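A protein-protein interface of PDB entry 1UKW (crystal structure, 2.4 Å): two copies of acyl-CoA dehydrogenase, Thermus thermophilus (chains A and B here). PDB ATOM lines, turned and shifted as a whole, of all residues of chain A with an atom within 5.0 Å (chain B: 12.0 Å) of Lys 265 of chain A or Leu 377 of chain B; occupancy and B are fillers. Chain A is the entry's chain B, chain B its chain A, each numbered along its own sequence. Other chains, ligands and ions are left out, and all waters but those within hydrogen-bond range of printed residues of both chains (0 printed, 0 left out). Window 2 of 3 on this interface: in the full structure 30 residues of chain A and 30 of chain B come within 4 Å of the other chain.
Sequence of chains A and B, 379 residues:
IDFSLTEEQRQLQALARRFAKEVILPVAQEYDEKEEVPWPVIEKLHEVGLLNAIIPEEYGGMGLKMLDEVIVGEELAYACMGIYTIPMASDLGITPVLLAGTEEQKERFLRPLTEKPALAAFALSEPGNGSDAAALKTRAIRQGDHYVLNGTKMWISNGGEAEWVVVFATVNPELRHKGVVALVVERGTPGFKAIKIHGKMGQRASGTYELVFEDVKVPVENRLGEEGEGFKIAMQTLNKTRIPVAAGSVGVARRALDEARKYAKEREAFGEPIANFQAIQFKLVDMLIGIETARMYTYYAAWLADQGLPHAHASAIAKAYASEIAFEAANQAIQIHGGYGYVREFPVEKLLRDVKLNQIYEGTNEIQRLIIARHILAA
O of Ile 376 of chain B sits at hydrogen-bond distance from NH1 of Arg 261 of chain A.
The backbone carbonyl oxygen (O) of Leu 377 of chain B is in hydrogen-bond range of the side-chain amino group (NZ) of Lys 265 of chain A (2.8 Å).
The backbone carbonyl oxygen (O) of Ala 275 of chain A sits at hydrogen-bond distance from the side-chain amide nitrogen (NE2) of Gln 281 of chain A, 2.9 Å away.
Among the printed residues, pairs that only touch across the chains: Leu 284 of chain A with Ile 376 of chain B (3.4 Å) and Gln 281 of chain A with Leu 377 of chain B (3.7 Å).
Lys 262 of chain A touches none of the printed residues of chain B.
No residue of chain B comes within 4 Å of Ala 264 of chain A.
Printed residues of chain B within 4 Å of Lys 265 of chain A: Leu 377.
No residue of chain B comes within 4 Å of Pro 273 of chain A.
Of chain B, only Leu 377 (3.7 Å) comes within 4 Å of Gln 281 of chain A.
Of the printed residues of chain B, Leu 284 of chain A touches Ile 376.
Ile 367 of chain B touches none of the printed residues of chain A.
Of the printed residues of chain A, Ile 376 of chain B touches Arg 261 and Leu 284.
Of the printed residues of chain A, Leu 377 of chain B touches Lys 265 (2.8 Å) and Gln 281 (3.7 Å).
The nearest printed residue of chain A that does not touch Ile 376 of chain B is Lys 265 of chain A (5.0 Å).
Printed residues of chain A that touch a printed residue of chain B: Arg 261, Lys 265, Gln 281 and Leu 284.
Among the printed residues, 4 pairs touch across the chains.
Among the printed residues, no Asp or Glu carboxylate lies within 4 Å of a Lys or Arg side-chain nitrogen of the other chain.
No position is printed for both chains.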
ATOM      1  N   ALA A 260     -19.826 -11.291  21.962  1.00  0.00           N
ATOM      2  CA  ALA A 260     -18.930 -10.656  21.004  1.00  0.00           C
ATOM      3  C   ALA A 260     -18.009 -11.643  20.294  1.00  0.00           C
ATOM      4  O   ALA A 260     -17.859 -11.594  19.076  1.00  0.00           O
ATOM      5  CB  ALA A 260     -18.092  -9.578  21.711  1.00  0.00           C
ATOM      6  N   ARG A 261     -17.387 -12.527  21.066  1.00  0.00           N
ATOM      7  CA  ARG A 261     -16.470 -13.516  20.519  1.00  0.00           C
ATOM      8  C   ARG A 261     -17.161 -14.543  19.626  1.00  0.00           C
ATOM      9  O   ARG A 261     -16.654 -14.880  18.557  1.00  0.00           O
ATOM     10  CB  ARG A 261     -15.741 -14.235  21.647  1.00  0.00           C
ATOM     11  CG  ARG A 261     -14.906 -15.398  21.180  1.00  0.00           C
ATOM     12  CD  ARG A 261     -14.115 -15.950  22.323  1.00  0.00           C
ATOM     13  NE  ARG A 261     -14.973 -16.255  23.457  1.00  0.00           N
ATOM     14  CZ  ARG A 261     -14.524 -16.496  24.682  1.00  0.00           C
ATOM     15  NH1 ARG A 261     -13.221 -16.471  24.938  1.00  0.00           N
ATOM     16  NH2 ARG A 261     -15.381 -16.756  25.658  1.00  0.00           N
ATOM     17  N   LYS A 262     -18.310 -15.043  20.076  1.00  0.00           N
ATOM     18  CA  LYS A 262     -19.075 -16.020  19.312  1.00  0.00           C
ATOM     19  C   LYS A 262     -19.489 -15.397  17.977  1.00  0.00           C
ATOM     20  O   LYS A 262     -19.460 -16.050  16.936  1.00  0.00           O
ATOM     21  CB  LYS A 262     -20.320 -16.442  20.092  1.00  0.00           C
ATOM     22  CG  LYS A 262     -21.221 -17.389  19.329  1.00  0.00           C
ATOM     23  CD  LYS A 262     -22.693 -17.096  19.586  1.00  0.00           C
ATOM     24  CE  LYS A 262     -23.131 -17.441  20.997  1.00  0.00           C
ATOM     25  NZ  LYS A 262     -24.578 -17.127  21.161  1.00  0.00           N
ATOM     26  N   TYR A 263     -19.862 -14.124  18.013  1.00  0.00           N
ATOM     27  CA  TYR A 263     -20.273 -13.425  16.803  1.00  0.00           C
ATOM     28  C   TYR A 263     -19.064 -13.146  15.915  1.00  0.00           C
ATOM     29  O   TYR A 263     -19.124 -13.316  14.695  1.00  0.00           O
ATOM     30  CB  TYR A 263     -20.963 -12.108  17.154  1.00  0.00           C
ATOM     31  CG  TYR A 263     -21.709 -11.500  15.997  1.00  0.00           C
ATOM     32  CD1 TYR A 263     -22.951 -12.005  15.597  1.00  0.00           C
ATOM     33  CD2 TYR A 263     -21.156 -10.450  15.266  1.00  0.00           C
ATOM     34  CE1 TYR A 263     -23.626 -11.475  14.487  1.00  0.00           C
ATOM     35  CE2 TYR A 263     -21.813  -9.918  14.162  1.00  0.00           C
ATOM     36  CZ  TYR A 263     -23.047 -10.434  13.773  1.00  0.00           C
ATOM     37  OH  TYR A 263     -23.678  -9.915  12.662  1.00  0.00           O
ATOM     38  N   ALA A 264     -17.966 -12.722  16.537  1.00  0.00           N
ATOM     39  CA  ALA A 264     -16.730 -12.409  15.817  1.00  0.00           C
ATOM     40  C   ALA A 264     -16.204 -13.600  15.020  1.00  0.00           C
ATOM     41  O   ALA A 264     -15.685 -13.431  13.913  1.00  0.00           O
ATOM     42  CB  ALA A 264     -15.659 -11.922  16.791  1.00  0.00           C
ATOM     43  N   LYS A 265     -16.337 -14.797  15.588  1.00  0.00           N
ATOM     44  CA  LYS A 265     -15.886 -16.023  14.933  1.00  0.00           C
ATOM     45  C   LYS A 265     -16.786 -16.432  13.775  1.00  0.00           C
ATOM     46  O   LYS A 265     -16.302 -16.896  12.747  1.00  0.00           O
ATOM     47  CB  LYS A 265     -15.845 -17.190  15.923  1.00  0.00           C
ATOM     48  CG  LYS A 265     -14.722 -17.163  16.937  1.00  0.00           C
ATOM     49  CD  LYS A 265     -14.884 -18.337  17.894  1.00  0.00           C
ATOM     50  CE  LYS A 265     -13.628 -18.575  18.706  1.00  0.00           C
ATOM     51  NZ  LYS A 265     -12.441 -18.768  17.806  1.00  0.00           N
ATOM     52  N   GLU A 266     -18.095 -16.268  13.946  1.00  0.00           N
ATOM     53  CA  GLU A 266     -19.057 -16.651  12.914  1.00  0.00           C
ATOM     54  C   GLU A 266     -19.256 -15.609  11.808  1.00  0.00           C
ATOM     55  O   GLU A 266     -19.343 -15.964  10.639  1.00  0.00           O
ATOM     56  CB  GLU A 266     -20.420 -16.954  13.540  1.00  0.00           C
ATOM     57  CG  GLU A 266     -20.371 -17.753  14.829  1.00  0.00           C
ATOM     58  CD  GLU A 266     -20.715 -19.225  14.647  1.00  0.00           C
ATOM     59  OE1 GLU A 266     -20.955 -19.913  15.680  1.00  0.00           O
ATOM     60  OE2 GLU A 266     -20.742 -19.692  13.479  1.00  0.00           O
ATOM     61  N   ARG A 267     -19.344 -14.331  12.176  1.00  0.00           N
ATOM     62  CA  ARG A 267     -19.565 -13.264  11.189  1.00  0.00           C
ATOM     63  C   ARG A 267     -18.324 -12.942  10.367  1.00  0.00           C
ATOM     64  O   ARG A 267     -17.244 -12.724  10.920  1.00  0.00           O
ATOM     65  CB  ARG A 267     -20.050 -11.992  11.882  1.00  0.00           C
ATOM     66  CG  ARG A 267     -20.334 -10.840  10.945  1.00  0.00           C
ATOM     67  CD  ARG A 267     -21.593 -11.055  10.114  1.00  0.00           C
ATOM     68  NE  ARG A 267     -21.988  -9.826   9.422  1.00  0.00           N
ATOM     69  CZ  ARG A 267     -23.132  -9.674   8.755  1.00  0.00           C
ATOM     70  NH1 ARG A 267     -24.001 -10.678   8.682  1.00  0.00           N
ATOM     71  NH2 ARG A 267     -23.418  -8.512   8.173  1.00  0.00           N
ATOM     72  N   PRO A 273     -13.514 -14.267   8.957  1.00  0.00           N
ATOM     73  CA  PRO A 273     -14.208 -14.016  10.226  1.00  0.00           C
ATOM     74  C   PRO A 273     -13.649 -12.708  10.799  1.00  0.00           C
ATOM     75  O   PRO A 273     -12.423 -12.518  10.842  1.00  0.00           O
ATOM     76  CB  PRO A 273     -13.828 -15.229  11.069  1.00  0.00           C
ATOM     77  CG  PRO A 273     -13.685 -16.301  10.051  1.00  0.00           C
ATOM     78  CD  PRO A 273     -12.920 -15.614   8.948  1.00  0.00           C
ATOM     79  N   ALA A 275     -13.206 -11.856  13.579  1.00  0.00           N
ATOM     80  CA  ALA A 275     -12.326 -12.154  14.698  1.00  0.00           C
ATOM     81  C   ALA A 275     -10.878 -12.145  14.228  1.00  0.00           C
ATOM     82  O   ALA A 275      -9.973 -11.945  15.025  1.00  0.00           O
ATOM     83  CB  ALA A 275     -12.670 -13.504  15.290  1.00  0.00           C
ATOM     84  N   GLN A 281      -9.905  -7.971  17.570  1.00  0.00           N
ATOM     85  CA  GLN A 281      -9.232  -8.795  18.560  1.00  0.00           C
ATOM     86  C   GLN A 281      -8.897  -7.955  19.789  1.00  0.00           C
ATOM     87  O   GLN A 281      -9.093  -8.387  20.925  1.00  0.00           O
ATOM     88  CB  GLN A 281      -7.952  -9.390  17.980  1.00  0.00           C
ATOM     89  CG  GLN A 281      -8.158 -10.166  16.691  1.00  0.00           C
ATOM     90  CD  GLN A 281      -6.951 -11.001  16.321  1.00  0.00           C
ATOM     91  OE1 GLN A 281      -5.807 -10.549  16.435  1.00  0.00           O
ATOM     92  NE2 GLN A 281      -7.197 -12.227  15.874  1.00  0.00           N
ATOM     93  N   LEU A 284     -11.797  -7.255  22.049  1.00  0.00           N
ATOM     94  CA  LEU A 284     -12.042  -8.442  22.862  1.00  0.00           C
ATOM     95  C   LEU A 284     -11.008  -8.568  23.979  1.00  0.00           C
ATOM     96  O   LEU A 284     -11.333  -8.967  25.101  1.00  0.00           O
ATOM     97  CB  LEU A 284     -12.019  -9.692  21.981  1.00  0.00           C
ATOM     98  CG  LEU A 284     -13.103  -9.770  20.903  1.00  0.00           C
ATOM     99  CD1 LEU A 284     -12.818 -10.950  19.989  1.00  0.00           C
ATOM    100  CD2 LEU A 284     -14.482  -9.908  21.544  1.00  0.00           C
ATOM    101  N   HIS B 313      -1.580 -15.965  29.617  1.00  0.00           N
ATOM    102  CA  HIS B 313      -2.553 -14.898  29.424  1.00  0.00           C
ATOM    103  C   HIS B 313      -2.616 -13.937  30.626  1.00  0.00           C
ATOM    104  O   HIS B 313      -2.682 -12.716  30.462  1.00  0.00           O
ATOM    105  CB  HIS B 313      -3.936 -15.508  29.167  1.00  0.00           C
ATOM    106  CG  HIS B 313      -4.552 -16.129  30.380  1.00  0.00           C
ATOM    107  ND1 HIS B 313      -3.945 -17.151  31.079  1.00  0.00           N
ATOM    108  CD2 HIS B 313      -5.687 -15.829  31.056  1.00  0.00           C
ATOM    109  CE1 HIS B 313      -4.677 -17.450  32.139  1.00  0.00           C
ATOM    110  NE2 HIS B 313      -5.739 -16.661  32.148  1.00  0.00           N
ATOM    111  N   ILE B 317      -1.702  -9.951  30.715  1.00  0.00           N
ATOM    112  CA  ILE B 317      -2.719  -9.000  31.154  1.00  0.00           C
ATOM    113  C   ILE B 317      -2.171  -8.101  32.266  1.00  0.00           C
ATOM    114  O   ILE B 317      -2.336  -6.885  32.222  1.00  0.00           O
ATOM    115  CB  ILE B 317      -4.007  -9.725  31.640  1.00  0.00           C
ATOM    116  CG1 ILE B 317      -4.774 -10.265  30.431  1.00  0.00           C
ATOM    117  CG2 ILE B 317      -4.883  -8.779  32.454  1.00  0.00           C
ATOM    118  CD1 ILE B 317      -6.017 -11.049  30.771  1.00  0.00           C
ATOM    119  N   GLU B 366       1.325  -4.388  22.769  1.00  0.00           N
ATOM    120  CA  GLU B 366       0.539  -4.810  21.606  1.00  0.00           C
ATOM    121  C   GLU B 366       0.631  -6.315  21.435  1.00  0.00           C
ATOM    122  O   GLU B 366      -0.371  -6.970  21.156  1.00  0.00           O
ATOM    123  CB  GLU B 366       1.014  -4.155  20.302  1.00  0.00           C
ATOM    124  CG  GLU B 366       0.545  -2.737  20.111  1.00  0.00           C
ATOM    125  CD  GLU B 366       1.222  -1.790  21.066  1.00  0.00           C
ATOM    126  OE1 GLU B 366       0.567  -0.817  21.501  1.00  0.00           O
ATOM    127  OE2 GLU B 366       2.410  -2.013  21.376  1.00  0.00           O
ATOM    128  N   ILE B 367       1.831  -6.870  21.589  1.00  0.00           N
ATOM    129  CA  ILE B 367       1.953  -8.302  21.446  1.00  0.00           C
ATOM    130  C   ILE B 367       1.421  -8.982  22.706  1.00  0.00           C
ATOM    131  O   ILE B 367       1.001 -10.140  22.652  1.00  0.00           O
ATOM    132  CB  ILE B 367       3.410  -8.743  21.102  1.00  0.00           C
ATOM    133  CG1 ILE B 367       4.300  -8.697  22.329  1.00  0.00           C
ATOM    134  CG2 ILE B 367       3.957  -7.887  19.953  1.00  0.00           C
ATOM    135  CD1 ILE B 367       4.293  -9.997  23.096  1.00  0.00           C
ATOM    136  N   GLN B 368       1.412  -8.264  23.834  1.00  0.00           N
ATOM    137  CA  GLN B 368       0.847  -8.832  25.062  1.00  0.00           C
ATOM    138  C   GLN B 368      -0.617  -9.064  24.698  1.00  0.00           C
ATOM    139  O   GLN B 368      -1.199 -10.093  25.036  1.00  0.00           O
ATOM    140  CB  GLN B 368       0.890  -7.853  26.251  1.00  0.00           C
ATOM    141  CG  GLN B 368       2.264  -7.399  26.737  1.00  0.00           C
ATOM    142  CD  GLN B 368       3.214  -8.545  27.030  1.00  0.00           C
ATOM    143  OE1 GLN B 368       2.841  -9.541  27.643  1.00  0.00           O
ATOM    144  NE2 GLN B 368       4.458  -8.398  26.597  1.00  0.00           N
ATOM    145  N   ARG B 369      -1.201  -8.085  24.008  1.00  0.00           N
ATOM    146  CA  ARG B 369      -2.593  -8.168  23.574  1.00  0.00           C
ATOM    147  C   ARG B 369      -2.799  -9.268  22.535  1.00  0.00           C
ATOM    148  O   ARG B 369      -3.847  -9.909  22.499  1.00  0.00           O
ATOM    149  CB  ARG B 369      -3.072  -6.820  23.029  1.00  0.00           C
ATOM    150  CG  ARG B 369      -3.341  -5.802  24.118  1.00  0.00           C
ATOM    151  CD  ARG B 369      -4.104  -4.609  23.600  1.00  0.00           C
ATOM    152  NE  ARG B 369      -4.658  -3.810  24.691  1.00  0.00           N
ATOM    153  CZ  ARG B 369      -3.952  -3.042  25.516  1.00  0.00           C
ATOM    154  NH1 ARG B 369      -2.636  -2.940  25.400  1.00  0.00           N
ATOM    155  NH2 ARG B 369      -4.575  -2.370  26.464  1.00  0.00           N
ATOM    156  N   LEU B 370      -1.796  -9.479  21.691  1.00  0.00           N
ATOM    157  CA  LEU B 370      -1.853 -10.534  20.691  1.00  0.00           C
ATOM    158  C   LEU B 370      -1.866 -11.880  21.420  1.00  0.00           C
ATOM    159  O   LEU B 370      -2.554 -12.814  21.012  1.00  0.00           O
ATOM    160  CB  LEU B 370      -0.643 -10.442  19.761  1.00  0.00           C
ATOM    161  CG  LEU B 370      -0.886  -9.791  18.394  1.00  0.00           C
ATOM    162  CD1 LEU B 370      -1.885  -8.662  18.506  1.00  0.00           C
ATOM    163  CD2 LEU B 370       0.439  -9.284  17.840  1.00  0.00           C
ATOM    164  N   ILE B 371      -1.106 -11.964  22.510  1.00  0.00           N
ATOM    165  CA  ILE B 371      -1.049 -13.183  23.312  1.00  0.00           C
ATOM    166  C   ILE B 371      -2.416 -13.473  23.933  1.00  0.00           C
ATOM    167  O   ILE B 371      -2.903 -14.604  23.882  1.00  0.00           O
ATOM    168  CB  ILE B 371       0.001 -13.055  24.431  1.00  0.00           C
ATOM    169  CG1 ILE B 371       1.401 -12.997  23.810  1.00  0.00           C
ATOM    170  CG2 ILE B 371      -0.133 -14.214  25.416  1.00  0.00           C
ATOM    171  CD1 ILE B 371       2.529 -12.837  24.805  1.00  0.00           C
ATOM    172  N   ILE B 372      -3.024 -12.444  24.518  1.00  0.00           N
ATOM    173  CA  ILE B 372      -4.332 -12.562  25.142  1.00  0.00           C
ATOM    174  C   ILE B 372      -5.370 -12.909  24.075  1.00  0.00           C
ATOM    175  O   ILE B 372      -6.237 -13.748  24.298  1.00  0.00           O
ATOM    176  CB  ILE B 372      -4.734 -11.241  25.845  1.00  0.00           C
ATOM    177  CG1 ILE B 372      -3.699 -10.893  26.914  1.00  0.00           C
ATOM    178  CG2 ILE B 372      -6.099 -11.376  26.484  1.00  0.00           C
ATOM    179  CD1 ILE B 372      -3.861  -9.515  27.514  1.00  0.00           C
ATOM    180  N   ALA B 373      -5.267 -12.270  22.912  1.00  0.00           N
ATOM    181  CA  ALA B 373      -6.193 -12.517  21.812  1.00  0.00           C
ATOM    182  C   ALA B 373      -6.197 -13.999  21.413  1.00  0.00           C
ATOM    183  O   ALA B 373      -7.259 -14.566  21.127  1.00  0.00           O
ATOM    184  CB  ALA B 373      -5.828 -11.642  20.600  1.00  0.00           C
ATOM    185  N   ARG B 374      -5.016 -14.624  21.399  1.00  0.00           N
ATOM    186  CA  ARG B 374      -4.915 -16.034  21.038  1.00  0.00           C
ATOM    187  C   ARG B 374      -5.601 -16.876  22.096  1.00  0.00           C
ATOM    188  O   ARG B 374      -6.302 -17.837  21.784  1.00  0.00           O
ATOM    189  CB  ARG B 374      -3.456 -16.448  20.894  1.00  0.00           C
ATOM    190  CG  ARG B 374      -2.743 -15.723  19.762  1.00  0.00           C
ATOM    191  CD  ARG B 374      -1.332 -16.262  19.552  1.00  0.00           C
ATOM    192  NE  ARG B 374      -0.549 -15.421  18.650  1.00  0.00           N
ATOM    193  CZ  ARG B 374       0.651 -15.744  18.176  1.00  0.00           C
ATOM    194  NH1 ARG B 374       1.214 -16.900  18.515  1.00  0.00           N
ATOM    195  NH2 ARG B 374       1.291 -14.909  17.365  1.00  0.00           N
ATOM    196  N   HIS B 375      -5.404 -16.498  23.350  1.00  0.00           N
ATOM    197  CA  HIS B 375      -6.028 -17.192  24.462  1.00  0.00           C
ATOM    198  C   HIS B 375      -7.556 -17.106  24.320  1.00  0.00           C
ATOM    199  O   HIS B 375      -8.272 -18.082  24.557  1.00  0.00           O
ATOM    200  CB  HIS B 375      -5.580 -16.545  25.782  1.00  0.00           C
ATOM    201  CG  HIS B 375      -6.299 -17.058  26.993  1.00  0.00           C
ATOM    202  ND1 HIS B 375      -6.035 -18.292  27.553  1.00  0.00           N
ATOM    203  CD2 HIS B 375      -7.291 -16.513  27.736  1.00  0.00           C
ATOM    204  CE1 HIS B 375      -6.834 -18.483  28.587  1.00  0.00           C
ATOM    205  NE2 HIS B 375      -7.606 -17.418  28.719  1.00  0.00           N
ATOM    206  N   ILE B 376      -8.047 -15.936  23.925  1.00  0.00           N
ATOM    207  CA  ILE B 376      -9.483 -15.723  23.781  1.00  0.00           C
ATOM    208  C   ILE B 376     -10.122 -16.482  22.626  1.00  0.00           C
ATOM    209  O   ILE B 376     -11.221 -17.015  22.761  1.00  0.00           O
ATOM    210  CB  ILE B 376      -9.822 -14.226  23.581  1.00  0.00           C
ATOM    211  CG1 ILE B 376      -9.337 -13.407  24.777  1.00  0.00           C
ATOM    212  CG2 ILE B 376     -11.328 -14.060  23.407  1.00  0.00           C
ATOM    213  CD1 ILE B 376      -9.664 -11.939  24.680  1.00  0.00           C
ATOM    214  N   LEU B 377      -9.437 -16.513  21.489  1.00  0.00           N
ATOM    215  CA  LEU B 377      -9.957 -17.173  20.301  1.00  0.00           C
ATOM    216  C   LEU B 377      -9.630 -18.651  20.196  1.00  0.00           C
ATOM    217  O   LEU B 377     -10.217 -19.345  19.375  1.00  0.00           O
ATOM    218  CB  LEU B 377      -9.462 -16.451  19.046  1.00  0.00           C
ATOM    219  CG  LEU B 377     -10.175 -15.174  18.571  1.00  0.00           C
ATOM    220  CD1 LEU B 377     -11.266 -14.762  19.543  1.00  0.00           C
ATOM    221  CD2 LEU B 377      -9.154 -14.069  18.396  1.00  0.00           C
ATOM    222  N   ALA B 378      -8.695 -19.125  21.017  1.00  0.00           N
ATOM    223  CA  ALA B 378      -8.295 -20.534  20.997  1.00  0.00           C
ATOM    224  C   ALA B 378      -9.530 -21.429  20.972  1.00  0.00           C
ATOM    225  O   ALA B 378     -10.295 -21.480  21.942  1.00  0.00           O
ATOM    226  CB  ALA B 378      -7.439 -20.860  22.217  1.00  0.00           C
ATOM    227  N   ALA B 379      -9.722 -22.131  19.859  1.00  0.00           N
ATOM    228  CA  ALA B 379     -10.877 -23.011  19.698  1.00  0.00           C
ATOM    229  C   ALA B 379     -10.800 -24.227  20.630  1.00  0.00           C
ATOM    230  O   ALA B 379     -11.105 -25.350  20.156  1.00  0.00           O
ATOM    231  CB  ALA B 379     -10.982 -23.470  18.224  1.00  0.00           C
ATOM    232  OXT ALA B 379     -10.454 -24.042  21.825  1.00  0.00           O
